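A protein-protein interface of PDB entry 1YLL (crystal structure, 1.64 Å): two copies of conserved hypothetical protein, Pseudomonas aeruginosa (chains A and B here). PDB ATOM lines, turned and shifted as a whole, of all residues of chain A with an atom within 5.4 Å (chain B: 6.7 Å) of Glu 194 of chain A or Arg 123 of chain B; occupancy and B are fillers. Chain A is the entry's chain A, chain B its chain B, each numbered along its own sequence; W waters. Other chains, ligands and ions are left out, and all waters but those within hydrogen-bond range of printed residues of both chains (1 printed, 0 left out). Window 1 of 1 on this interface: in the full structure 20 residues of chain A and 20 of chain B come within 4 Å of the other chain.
NE of Arg 121 of chain A lies within salt-bridge range of OD2 of Asp 196 of chain B, 3.1 Å away.
The side-chain carboxylate of Glu 194 of chain B is in salt-bridge range of the guanidinium group of Arg 123 of chain A (2.9 Å).
N of Thr 138 of chain A lies within hydrogen-bond range of O of Ala 122 of chain B (3.0 Å).
The side-chain carboxylate of Glu 194 of chain A is in salt-bridge range of the guanidinium group of Arg 123 of chain B, 2.9 Å away.
OD2 of Asp 196 of chain A lies within salt-bridge range of NE of Arg 121 of chain B, at 3.8 Å.
NH1 of Arg 121 of chain B lies close to NH2 of Arg 121 of chain A, at 3.2 Å.
The backbone carbonyl oxygen (O) of His 136 of chain A sits at hydrogen-bond distance from the backbone NH (N) of Leu 124 of chain B (2.9 Å).
Among the printed residues, pairs that only touch across the chains: Arg 123 of chain A with Arg 123 of chain B, Gln 125 of chain A with Leu 127 of chain B, Leu 127 of chain A with Gln 125 of chain B, Trp 135 of chain A with Arg 123 of chain B, Trp 135 of chain A with Leu 124 of chain B, Trp 135 of chain A with Gln 125 of chain B, His 136 of chain A with Arg 123 of chain B, Gly 137 of chain A with Ala 122 of chain B, Gly 137 of chain A with Arg 123 of chain B and Thr 138 of chain A with Tyr 115 of chain B.
Leu 142 of chain A touches none of the printed residues of chain B.
Glu 194 of chain A touches one residue of chain B.
Ile 64 of chain B touches none of the printed residues of chain A.
Printed residues of chain A within 4 Å of Arg 121 of chain B: Arg 121 (3.2 Å) and Asp 196 (3.6 Å).
Of the printed residues of chain A, Arg 123 of chain B touches Arg 123, Trp 135, His 136, Gly 137 and Glu 194.
Printed residues of chain A within 4 Å of Leu 124 of chain B: Trp 135 and His 136.
Of the printed residues of chain A, Gln 125 of chain B touches Leu 127 (3.9 Å) and Trp 135 (3.7 Å).
Of the printed residues of chain A, Glu 194 of chain B touches Arg 123 (2.9 Å).
Of the printed residues of chain A, Asp 196 of chain B touches Arg 121 (3.1 Å).
The nearest residue of chain B that does not touch Glu 194 of chain A is Gln 125 of chain B (5.9 Å).
The nearest printed residue of chain A that does not touch Arg 123 of chain B is Gln 125 of chain A (4.7 Å).
The nearest printed residue of chain B that does not touch Thr 138 of chain A is Arg 121 of chain B (4.4 Å).
Of the 19 printed residues of chain A, 10 touch a printed residue of chain B.
Of the 14 printed residues of chain B, 9 touch a printed residue of chain A.
Printed residues of chain B that touch a printed residue of chain A: Tyr 115, Arg 121, Ala 122, Arg 123, Leu 124, Gln 125, Leu 127, Glu 194 and Asp 196.
Hydrophobic or aromatic side chains of chain B that line the printed part of chain A: Tyr 115 and Leu 127.
Among the printed residues, 17 pairs touch across the chains.
Among the printed residues, Asp or Glu carboxylates within 4 Å of a Lys or Arg side-chain nitrogen of the other chain: Arg 121 of chain A with Asp 196 of chain B (3.1 Å), Arg 123 of chain A with Glu 194 of chain B (2.9 Å), Glu 194 of chain A with Arg 123 of chain B (2.9 Å) and Asp 196 of chain A with Arg 121 of chain B (3.8 Å).
Water W1 bridges the backbone carbonyl oxygen of Leu 124 of chain B (2.9 Å) and the backbone NH of His 136 of chain A (3.4 Å).
Arg 121 of chain A touches Asp 196 of chain B, and with the chains exchanged Asp 196 of chain A touches Arg 121 of chain B.
Arg 123 of chain B touches its own counterpart, Arg 123 of chain A.
Arg 123 of chain A touches Glu 194 of chain B, and with the chains exchanged Glu 194 of chain A touches Arg 123 of chain B.
Gln 125 of chain A touches Leu 127 of chain B, and with the chains exchanged Leu 127 of chain A touches Gln 125 of chain B.
Positions printed for both chains: 121, 122, 123, 124, 125, 127, 192, 193, 194, 195 and 196.
Of the 17 pairs that touch across the chains among the printed residues, 8 have their exchanged pair printed and touching as well.
The guanidinium group (NH2) of Arg 121 of chain A lies within salt-bridge range of the side-chain carboxylate (OD1) of Asp 196 of chain A.
N of Gln 125 of chain B lies within hydrogen-bond range of O of Ala 192 of chain B.
The backbone carbonyl oxygen of Gln 125 of chain A sits at hydrogen-bond distance from the backbone NH of Ala 192 of chain A, at 2.9 Å.
OE1 of Gln 125 of chain B lies within hydrogen-bond range of NH1 of Arg 123 of chain B (2.9 Å).
The guanidinium group (NH1) of Arg 123 of chain A sits at hydrogen-bond distance from the side-chain amide oxygen (OE1) of Gln 125 of chain A, at 2.9 Å.
The backbone NH of Arg 123 of chain A lies within hydrogen-bond range of the backbone carbonyl oxygen of Glu 194 of chain A, at 2.9 Å.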
ATOM      1  N   ARG A 121      24.103   1.464  -7.650  1.00  0.00           N
ATOM      2  CA  ARG A 121      24.026   2.199  -8.922  1.00  0.00           C
ATOM      3  C   ARG A 121      24.866   3.442  -8.654  1.00  0.00           C
ATOM      4  O   ARG A 121      24.740   4.052  -7.605  1.00  0.00           O
ATOM      5  CB  ARG A 121      22.588   2.563  -9.280  1.00  0.00           C
ATOM      6  CG  ARG A 121      21.952   1.558 -10.246  1.00  0.00           C
ATOM      7  CD  ARG A 121      20.545   1.939 -10.687  1.00  0.00           C
ATOM      8  NE  ARG A 121      20.460   3.319 -11.156  1.00  0.00           N
ATOM      9  CZ  ARG A 121      20.267   4.358 -10.346  1.00  0.00           C
ATOM     10  NH1 ARG A 121      20.206   5.592 -10.830  1.00  0.00           N
ATOM     11  NH2 ARG A 121      20.122   4.159  -9.043  1.00  0.00           N
ATOM     12  N   ALA A 122      25.706   3.811  -9.617  1.00  0.00           N
ATOM     13  CA  ALA A 122      26.675   4.903  -9.448  1.00  0.00           C
ATOM     14  C   ALA A 122      26.668   5.959 -10.541  1.00  0.00           C
ATOM     15  O   ALA A 122      26.301   5.685 -11.685  1.00  0.00           O
ATOM     16  CB  ALA A 122      28.095   4.323  -9.368  1.00  0.00           C
ATOM     17  N   ARG A 123      27.134   7.156 -10.174  1.00  0.00           N
ATOM     18  CA  ARG A 123      27.267   8.255 -11.135  1.00  0.00           C
ATOM     19  C   ARG A 123      28.527   8.993 -10.694  1.00  0.00           C
ATOM     20  O   ARG A 123      28.752   9.148  -9.501  1.00  0.00           O
ATOM     21  CB  ARG A 123      26.084   9.220 -11.049  1.00  0.00           C
ATOM     22  CG  ARG A 123      26.042  10.180 -12.222  1.00  0.00           C
ATOM     23  CD  ARG A 123      24.887  11.177 -12.103  1.00  0.00           C
ATOM     24  NE  ARG A 123      24.729  11.994 -13.315  1.00  0.00           N
ATOM     25  CZ  ARG A 123      25.482  13.050 -13.601  1.00  0.00           C
ATOM     26  NH1 ARG A 123      26.443  13.418 -12.768  1.00  0.00           N
ATOM     27  NH2 ARG A 123      25.264  13.726 -14.730  1.00  0.00           N
ATOM     28  N   LEU A 124      29.352   9.420 -11.653  1.00  0.00           N
ATOM     29  CA  LEU A 124      30.569  10.126 -11.297  1.00  0.00           C
ATOM     30  C   LEU A 124      30.741  11.248 -12.297  1.00  0.00           C
ATOM     31  O   LEU A 124      30.690  11.015 -13.501  1.00  0.00           O
ATOM     32  CB  LEU A 124      31.796   9.181 -11.313  1.00  0.00           C
ATOM     33  CG  LEU A 124      33.098   9.825 -10.819  1.00  0.00           C
ATOM     34  CD1 LEU A 124      34.043   8.780 -10.210  1.00  0.00           C
ATOM     35  CD2 LEU A 124      33.770  10.520 -12.046  1.00  0.00           C
ATOM     36  N   GLN A 125      30.886  12.472 -11.812  1.00  0.00           N
ATOM     37  CA  GLN A 125      31.101  13.551 -12.777  1.00  0.00           C
ATOM     38  C   GLN A 125      31.991  14.655 -12.228  1.00  0.00           C
ATOM     39  O   GLN A 125      31.741  15.148 -11.124  1.00  0.00           O
ATOM     40  CB  GLN A 125      29.780  14.198 -13.194  1.00  0.00           C
ATOM     41  CG  GLN A 125      29.976  15.306 -14.236  1.00  0.00           C
ATOM     42  CD  GLN A 125      28.704  15.796 -14.876  1.00  0.00           C
ATOM     43  OE1 GLN A 125      27.590  15.542 -14.395  1.00  0.00           O
ATOM     44  NE2 GLN A 125      28.857  16.564 -15.960  1.00  0.00           N
ATOM     45  N   LEU A 127      33.116  18.432 -12.105  1.00  0.00           N
ATOM     46  CA  LEU A 127      32.381  19.677 -12.365  1.00  0.00           C
ATOM     47  C   LEU A 127      33.287  20.813 -11.927  1.00  0.00           C
ATOM     48  O   LEU A 127      33.953  20.684 -10.917  1.00  0.00           O
ATOM     49  CB  LEU A 127      31.145  19.732 -11.479  1.00  0.00           C
ATOM     50  CG  LEU A 127      30.092  18.636 -11.717  1.00  0.00           C
ATOM     51  CD1 LEU A 127      29.060  18.647 -10.565  1.00  0.00           C
ATOM     52  CD2 LEU A 127      29.394  18.870 -13.055  1.00  0.00           C
ATOM     53  N   TRP A 135      22.220  21.298  -8.573  1.00  0.00           N
ATOM     54  CA  TRP A 135      21.489  20.214  -9.231  1.00  0.00           C
ATOM     55  C   TRP A 135      20.502  19.649  -8.220  1.00  0.00           C
ATOM     56  O   TRP A 135      20.582  19.943  -7.029  1.00  0.00           O
ATOM     57  CB  TRP A 135      22.404  19.075  -9.752  1.00  0.00           C
ATOM     58  CG  TRP A 135      23.017  18.154  -8.727  1.00  0.00           C
ATOM     59  CD1 TRP A 135      22.495  16.958  -8.266  1.00  0.00           C
ATOM     60  CD2 TRP A 135      24.245  18.352  -8.017  1.00  0.00           C
ATOM     61  NE1 TRP A 135      23.343  16.410  -7.317  1.00  0.00           N
ATOM     62  CE2 TRP A 135      24.412  17.254  -7.139  1.00  0.00           C
ATOM     63  CE3 TRP A 135      25.219  19.344  -8.044  1.00  0.00           C
ATOM     64  CZ2 TRP A 135      25.517  17.137  -6.283  1.00  0.00           C
ATOM     65  CZ3 TRP A 135      26.332  19.220  -7.196  1.00  0.00           C
ATOM     66  CH2 TRP A 135      26.460  18.132  -6.335  1.00  0.00           C
ATOM     67  N   HIS A 136      19.552  18.867  -8.722  1.00  0.00           N
ATOM     68  CA  HIS A 136      18.586  18.177  -7.854  1.00  0.00           C
ATOM     69  C   HIS A 136      18.787  16.694  -8.109  1.00  0.00           C
ATOM     70  O   HIS A 136      18.950  16.297  -9.244  1.00  0.00           O
ATOM     71  CB  HIS A 136      17.163  18.549  -8.239  1.00  0.00           C
ATOM     72  CG  HIS A 136      16.811  19.976  -7.948  1.00  0.00           C
ATOM     73  ND1 HIS A 136      15.996  20.360  -6.898  1.00  0.00           N
ATOM     74  CD2 HIS A 136      17.137  21.111  -8.604  1.00  0.00           C
ATOM     75  CE1 HIS A 136      15.833  21.674  -6.926  1.00  0.00           C
ATOM     76  NE2 HIS A 136      16.511  22.152  -7.957  1.00  0.00           N
ATOM     77  N   GLY A 137      18.778  15.874  -7.059  1.00  0.00           N
ATOM     78  CA  GLY A 137      18.917  14.443  -7.296  1.00  0.00           C
ATOM     79  C   GLY A 137      18.371  13.668  -6.133  1.00  0.00           C
ATOM     80  O   GLY A 137      18.382  14.178  -5.027  1.00  0.00           O
ATOM     81  N   THR A 138      17.969  12.428  -6.395  1.00  0.00           N
ATOM     82  CA  THR A 138      17.402  11.566  -5.379  1.00  0.00           C
ATOM     83  C   THR A 138      18.386  10.590  -4.769  1.00  0.00           C
ATOM     84  O   THR A 138      18.032   9.842  -3.878  1.00  0.00           O
ATOM     85  CB  THR A 138      16.223  10.790  -5.955  1.00  0.00           C
ATOM     86  OG1 THR A 138      15.258  11.720  -6.465  1.00  0.00           O
ATOM     87  CG2 THR A 138      15.577   9.930  -4.889  1.00  0.00           C
ATOM     88  N   ALA A 139      19.632  10.598  -5.233  1.00  0.00           N
ATOM     89  CA  ALA A 139      20.642   9.693  -4.701  1.00  0.00           C
ATOM     90  C   ALA A 139      20.692   9.739  -3.182  1.00  0.00           C
ATOM     91  O   ALA A 139      20.689  10.823  -2.577  1.00  0.00           O
ATOM     92  CB  ALA A 139      22.034  10.048  -5.278  1.00  0.00           C
ATOM     93  N   THR A 141      23.197   8.443  -1.378  1.00  0.00           N
ATOM     94  CA  THR A 141      24.566   8.715  -0.981  1.00  0.00           C
ATOM     95  C   THR A 141      25.235   9.668  -1.964  1.00  0.00           C
ATOM     96  O   THR A 141      25.140   9.478  -3.169  1.00  0.00           O
ATOM     97  CB  THR A 141      25.396   7.407  -0.920  1.00  0.00           C
ATOM     98  OG1 THR A 141      24.981   6.622   0.207  1.00  0.00           O
ATOM     99  CG2 THR A 141      26.882   7.696  -0.768  1.00  0.00           C
ATOM    100  N   LEU A 142      25.836  10.724  -1.429  1.00  0.00           N
ATOM    101  CA  LEU A 142      26.604  11.666  -2.238  1.00  0.00           C
ATOM    102  C   LEU A 142      27.970  11.860  -1.602  1.00  0.00           C
ATOM    103  O   LEU A 142      28.093  12.079  -0.390  1.00  0.00           O
ATOM    104  CB  LEU A 142      25.941  13.045  -2.357  1.00  0.00           C
ATOM    105  CG  LEU A 142      26.838  14.151  -2.979  1.00  0.00           C
ATOM    106  CD1 LEU A 142      27.107  13.879  -4.491  1.00  0.00           C
ATOM    107  CD2 LEU A 142      26.148  15.536  -2.854  1.00  0.00           C
ATOM    108  N   LEU A 143      29.002  11.738  -2.429  1.00  0.00           N
ATOM    109  CA  LEU A 143      30.344  12.024  -2.001  1.00  0.00           C
ATOM    110  C   LEU A 143      30.751  13.187  -2.900  1.00  0.00           C
ATOM    111  O   LEU A 143      30.705  13.072  -4.114  1.00  0.00           O
ATOM    112  CB  LEU A 143      31.256  10.828  -2.241  1.00  0.00           C
ATOM    113  CG  LEU A 143      31.031   9.633  -1.324  1.00  0.00           C
ATOM    114  CD1 LEU A 143      31.328   8.350  -2.099  1.00  0.00           C
ATOM    115  CD2 LEU A 143      31.949   9.735  -0.111  1.00  0.00           C
ATOM    116  N   ALA A 192      31.637  14.879  -8.242  1.00  0.00           N
ATOM    117  CA  ALA A 192      30.409  14.436  -7.584  1.00  0.00           C
ATOM    118  C   ALA A 192      30.193  12.953  -7.876  1.00  0.00           C
ATOM    119  O   ALA A 192      30.035  12.557  -9.021  1.00  0.00           O
ATOM    120  CB  ALA A 192      29.209  15.242  -8.103  1.00  0.00           C
ATOM    121  N   VAL A 193      30.141  12.164  -6.805  1.00  0.00           N
ATOM    122  CA  VAL A 193      29.930  10.732  -6.885  1.00  0.00           C
ATOM    123  C   VAL A 193      28.621  10.413  -6.171  1.00  0.00           C
ATOM    124  O   VAL A 193      28.437  10.728  -4.982  1.00  0.00           O
ATOM    125  CB  VAL A 193      31.086   9.994  -6.219  1.00  0.00           C
ATOM    126  CG1 VAL A 193      30.830   8.473  -6.255  1.00  0.00           C
ATOM    127  CG2 VAL A 193      32.406  10.322  -6.987  1.00  0.00           C
ATOM    128  N   GLU A 194      27.694   9.815  -6.905  1.00  0.00           N
ATOM    129  CA  GLU A 194      26.405   9.492  -6.318  1.00  0.00           C
ATOM    130  C   GLU A 194      26.196   8.002  -6.386  1.00  0.00           C
ATOM    131  O   GLU A 194      26.502   7.346  -7.396  1.00  0.00           O
ATOM    132  CB  GLU A 194      25.295  10.250  -7.048  1.00  0.00           C
ATOM    133  CG  GLU A 194      25.425  11.760  -6.851  1.00  0.00           C
ATOM    134  CD  GLU A 194      24.680  12.562  -7.898  1.00  0.00           C
ATOM    135  OE1 GLU A 194      25.321  13.430  -8.542  1.00  0.00           O
ATOM    136  OE2 GLU A 194      23.473  12.318  -8.077  1.00  0.00           O
ATOM    137  N   LEU A 195      25.670   7.458  -5.292  1.00  0.00           N
ATOM    138  CA  LEU A 195      25.430   6.025  -5.208  1.00  0.00           C
ATOM    139  C   LEU A 195      24.064   5.744  -4.609  1.00  0.00           C
ATOM    140  O   LEU A 195      23.564   6.492  -3.779  1.00  0.00           O
ATOM    141  CB  LEU A 195      26.506   5.361  -4.337  1.00  0.00           C
ATOM    142  CG  LEU A 195      27.936   5.509  -4.908  1.00  0.00           C
ATOM    143  CD1 LEU A 195      28.967   5.662  -3.812  1.00  0.00           C
ATOM    144  CD2 LEU A 195      28.237   4.279  -5.772  1.00  0.00           C
ATOM    145  N   ASP A 196      23.453   4.674  -5.082  1.00  0.00           N
ATOM    146  CA  ASP A 196      22.173   4.198  -4.527  1.00  0.00           C
ATOM    147  C   ASP A 196      22.313   2.719  -4.321  1.00  0.00           C
ATOM    148  O   ASP A 196      22.962   2.051  -5.100  1.00  0.00           O
ATOM    149  CB  ASP A 196      21.013   4.459  -5.466  1.00  0.00           C
ATOM    150  CG  ASP A 196      20.390   5.804  -5.222  1.00  0.00           C
ATOM    151  OD1 ASP A 196      20.352   6.604  -6.168  1.00  0.00           O
ATOM    152  OD2 ASP A 196      19.942   6.067  -4.081  1.00  0.00           O
ATOM    153  N   ILE B  64       9.821  19.683 -11.157  1.00  0.00           N
ATOM    154  CA  ILE B  64      11.031  20.512 -11.144  1.00  0.00           C
ATOM    155  C   ILE B  64      10.856  21.405 -12.380  1.00  0.00           C
ATOM    156  O   ILE B  64      10.713  20.916 -13.519  1.00  0.00           O
ATOM    157  CB  ILE B  64      12.361  19.729 -11.279  1.00  0.00           C
ATOM    158  CG1 ILE B  64      12.459  18.623 -10.222  1.00  0.00           C
ATOM    159  CG2 ILE B  64      13.535  20.739 -11.109  1.00  0.00           C
ATOM    160  CD1 ILE B  64      13.720  17.759 -10.370  1.00  0.00           C
ATOM    161  N   LEU B 113       9.908  19.027 -15.613  1.00  0.00           N
ATOM    162  CA  LEU B 113       9.945  17.576 -15.398  1.00  0.00           C
ATOM    163  C   LEU B 113       8.865  17.288 -14.375  1.00  0.00           C
ATOM    164  O   LEU B 113       8.782  17.978 -13.361  1.00  0.00           O
ATOM    165  CB  LEU B 113      11.262  17.153 -14.755  1.00  0.00           C
ATOM    166  CG  LEU B 113      11.810  15.722 -14.815  1.00  0.00           C
ATOM    167  CD1 LEU B 113      12.397  15.329 -13.501  1.00  0.00           C
ATOM    168  CD2 LEU B 113      10.876  14.749 -15.414  1.00  0.00           C
ATOM    169  N   TYR B 115       7.353  13.882 -12.295  1.00  0.00           N
ATOM    170  CA  TYR B 115       7.558  12.444 -12.199  1.00  0.00           C
ATOM    171  C   TYR B 115       6.979  11.869 -10.921  1.00  0.00           C
ATOM    172  O   TYR B 115       6.806  12.577  -9.938  1.00  0.00           O
ATOM    173  CB  TYR B 115       9.061  12.106 -12.325  1.00  0.00           C
ATOM    174  CG  TYR B 115       9.931  12.485 -11.146  1.00  0.00           C
ATOM    175  CD1 TYR B 115      10.179  11.581 -10.101  1.00  0.00           C
ATOM    176  CD2 TYR B 115      10.467  13.759 -11.040  1.00  0.00           C
ATOM    177  CE1 TYR B 115      10.918  11.936  -8.998  1.00  0.00           C
ATOM    178  CE2 TYR B 115      11.214  14.132  -9.938  1.00  0.00           C
ATOM    179  CZ  TYR B 115      11.434  13.229  -8.915  1.00  0.00           C
ATOM    180  OH  TYR B 115      12.116  13.580  -7.798  1.00  0.00           O
ATOM    181  N   ARG B 121      13.438   7.320  -9.577  1.00  0.00           N
ATOM    182  CA  ARG B 121      14.436   8.105  -8.879  1.00  0.00           C
ATOM    183  C   ARG B 121      14.742   9.136  -9.986  1.00  0.00           C
ATOM    184  O   ARG B 121      14.583   8.835 -11.159  1.00  0.00           O
ATOM    185  CB  ARG B 121      15.674   7.273  -8.590  1.00  0.00           C
ATOM    186  CG  ARG B 121      15.500   6.159  -7.535  1.00  0.00           C
ATOM    187  CD  ARG B 121      16.846   5.895  -6.874  1.00  0.00           C
ATOM    188  NE  ARG B 121      16.835   4.806  -5.900  1.00  0.00           N
ATOM    189  CZ  ARG B 121      17.140   3.544  -6.187  1.00  0.00           C
ATOM    190  NH1 ARG B 121      17.479   3.206  -7.424  1.00  0.00           N
ATOM    191  NH2 ARG B 121      17.128   2.627  -5.230  1.00  0.00           N
ATOM    192  N   ALA B 122      15.196  10.335  -9.624  1.00  0.00           N
ATOM    193  CA  ALA B 122      15.418  11.367 -10.634  1.00  0.00           C
ATOM    194  C   ALA B 122      16.588  12.270 -10.329  1.00  0.00           C
ATOM    195  O   ALA B 122      16.917  12.489  -9.182  1.00  0.00           O
ATOM    196  CB  ALA B 122      14.152  12.217 -10.763  1.00  0.00           C
ATOM    197  N   ARG B 123      17.217  12.803 -11.369  1.00  0.00           N
ATOM    198  CA  ARG B 123      18.312  13.738 -11.175  1.00  0.00           C
ATOM    199  C   ARG B 123      18.138  14.748 -12.319  1.00  0.00           C
ATOM    200  O   ARG B 123      17.755  14.380 -13.423  1.00  0.00           O
ATOM    201  CB  ARG B 123      19.657  13.040 -11.312  1.00  0.00           C
ATOM    202  CG  ARG B 123      20.844  13.922 -10.928  1.00  0.00           C
ATOM    203  CD  ARG B 123      22.183  13.203 -11.224  1.00  0.00           C
ATOM    204  NE  ARG B 123      23.283  13.942 -10.611  1.00  0.00           N
ATOM    205  CZ  ARG B 123      23.839  15.019 -11.159  1.00  0.00           C
ATOM    206  NH1 ARG B 123      23.392  15.464 -12.334  1.00  0.00           N
ATOM    207  NH2 ARG B 123      24.830  15.660 -10.518  1.00  0.00           N
ATOM    208  N   LEU B 124      18.418  16.019 -12.051  1.00  0.00           N
ATOM    209  CA  LEU B 124      18.263  16.999 -13.102  1.00  0.00           C
ATOM    210  C   LEU B 124      19.349  18.036 -12.912  1.00  0.00           C
ATOM    211  O   LEU B 124      19.521  18.548 -11.834  1.00  0.00           O
ATOM    212  CB  LEU B 124      16.886  17.667 -13.029  1.00  0.00           C
ATOM    213  CG  LEU B 124      16.542  18.755 -14.069  1.00  0.00           C
ATOM    214  CD1 LEU B 124      15.035  18.882 -14.344  1.00  0.00           C
ATOM    215  CD2 LEU B 124      17.100  20.083 -13.564  1.00  0.00           C
ATOM    216  N   GLN B 125      20.108  18.303 -13.962  1.00  0.00           N
ATOM    217  CA  GLN B 125      21.150  19.319 -13.826  1.00  0.00           C
ATOM    218  C   GLN B 125      21.435  20.081 -15.109  1.00  0.00           C
ATOM    219  O   GLN B 125      21.666  19.469 -16.164  1.00  0.00           O
ATOM    220  CB  GLN B 125      22.476  18.685 -13.395  1.00  0.00           C
ATOM    221  CG  GLN B 125      23.604  19.718 -13.217  1.00  0.00           C
ATOM    222  CD  GLN B 125      24.844  19.105 -12.550  1.00  0.00           C
ATOM    223  OE1 GLN B 125      24.988  17.889 -12.448  1.00  0.00           O
ATOM    224  NE2 GLN B 125      25.753  19.956 -12.123  1.00  0.00           N
ATOM    225  N   LEU B 127      23.831  22.086 -17.464  1.00  0.00           N
ATOM    226  CA  LEU B 127      25.267  22.015 -17.714  1.00  0.00           C
ATOM    227  C   LEU B 127      25.593  22.834 -18.954  1.00  0.00           C
ATOM    228  O   LEU B 127      24.864  22.765 -19.949  1.00  0.00           O
ATOM    229  CB  LEU B 127      25.686  20.559 -17.996  1.00  0.00           C
ATOM    230  CG  LEU B 127      25.469  19.470 -16.930  1.00  0.00           C
ATOM    231  CD1 LEU B 127      25.526  18.060 -17.597  1.00  0.00           C
ATOM    232  CD2 LEU B 127      26.478  19.618 -15.813  1.00  0.00           C
ATOM    233  N   ALA B 192      20.501  17.822 -18.269  1.00  0.00           N
ATOM    234  CA  ALA B 192      20.581  16.366 -18.191  1.00  0.00           C
ATOM    235  C   ALA B 192      19.602  15.876 -17.138  1.00  0.00           C
ATOM    236  O   ALA B 192      19.742  16.238 -15.956  1.00  0.00           O
ATOM    237  CB  ALA B 192      22.012  15.955 -17.846  1.00  0.00           C
ATOM    238  N   VAL B 193      18.611  15.081 -17.576  1.00  0.00           N
ATOM    239  CA  VAL B 193      17.583  14.535 -16.683  1.00  0.00           C
ATOM    240  C   VAL B 193      17.782  13.026 -16.708  1.00  0.00           C
ATOM    241  O   VAL B 193      17.738  12.385 -17.750  1.00  0.00           O
ATOM    242  CB  VAL B 193      16.167  14.892 -17.215  1.00  0.00           C
ATOM    243  CG1 VAL B 193      15.084  14.255 -16.338  1.00  0.00           C
ATOM    244  CG2 VAL B 193      16.000  16.382 -17.218  1.00  0.00           C
ATOM    245  N   GLU B 194      18.025  12.459 -15.534  1.00  0.00           N
ATOM    246  CA  GLU B 194      18.260  11.020 -15.430  1.00  0.00           C
ATOM    247  C   GLU B 194      17.172  10.423 -14.574  1.00  0.00           C
ATOM    248  O   GLU B 194      16.829  10.971 -13.545  1.00  0.00           O
ATOM    249  CB  GLU B 194      19.683  10.778 -14.867  1.00  0.00           C
ATOM    250  CG  GLU B 194      20.772  11.175 -15.907  1.00  0.00           C
ATOM    251  CD  GLU B 194      22.167  11.440 -15.316  1.00  0.00           C
ATOM    252  OE1 GLU B 194      22.687  12.572 -15.450  1.00  0.00           O
ATOM    253  OE2 GLU B 194      22.749  10.511 -14.749  1.00  0.00           O
ATOM    254  N   LEU B 195      16.606   9.304 -15.030  1.00  0.00           N
ATOM    255  CA  LEU B 195      15.558   8.667 -14.265  1.00  0.00           C
ATOM    256  C   LEU B 195      15.858   7.172 -14.149  1.00  0.00           C
ATOM    257  O   LEU B 195      16.417   6.561 -15.044  1.00  0.00           O
ATOM    258  CB  LEU B 195      14.209   8.896 -14.968  1.00  0.00           C
ATOM    259  CG  LEU B 195      13.779  10.369 -15.138  1.00  0.00           C
ATOM    260  CD1 LEU B 195      12.863  10.567 -16.343  1.00  0.00           C
ATOM    261  CD2 LEU B 195      13.120  10.822 -13.872  1.00  0.00           C
ATOM    262  N   ASP B 196      15.494   6.590 -13.027  1.00  0.00           N
ATOM    263  CA  ASP B 196      15.687   5.163 -12.928  1.00  0.00           C
ATOM    264  C   ASP B 196      14.469   4.564 -12.265  1.00  0.00           C
ATOM    265  O   ASP B 196      13.809   5.207 -11.469  1.00  0.00           O
ATOM    266  CB  ASP B 196      16.962   4.831 -12.165  1.00  0.00           C
ATOM    267  CG  ASP B 196      17.348   3.365 -12.305  1.00  0.00           C
ATOM    268  OD1 ASP B 196      16.817   2.540 -11.532  1.00  0.00           O
ATOM    269  OD2 ASP B 196      18.156   3.034 -13.203  1.00  0.00           O
HETATM  270  O   HOH W   1      18.761  21.205 -10.993  1.00  0.00           O
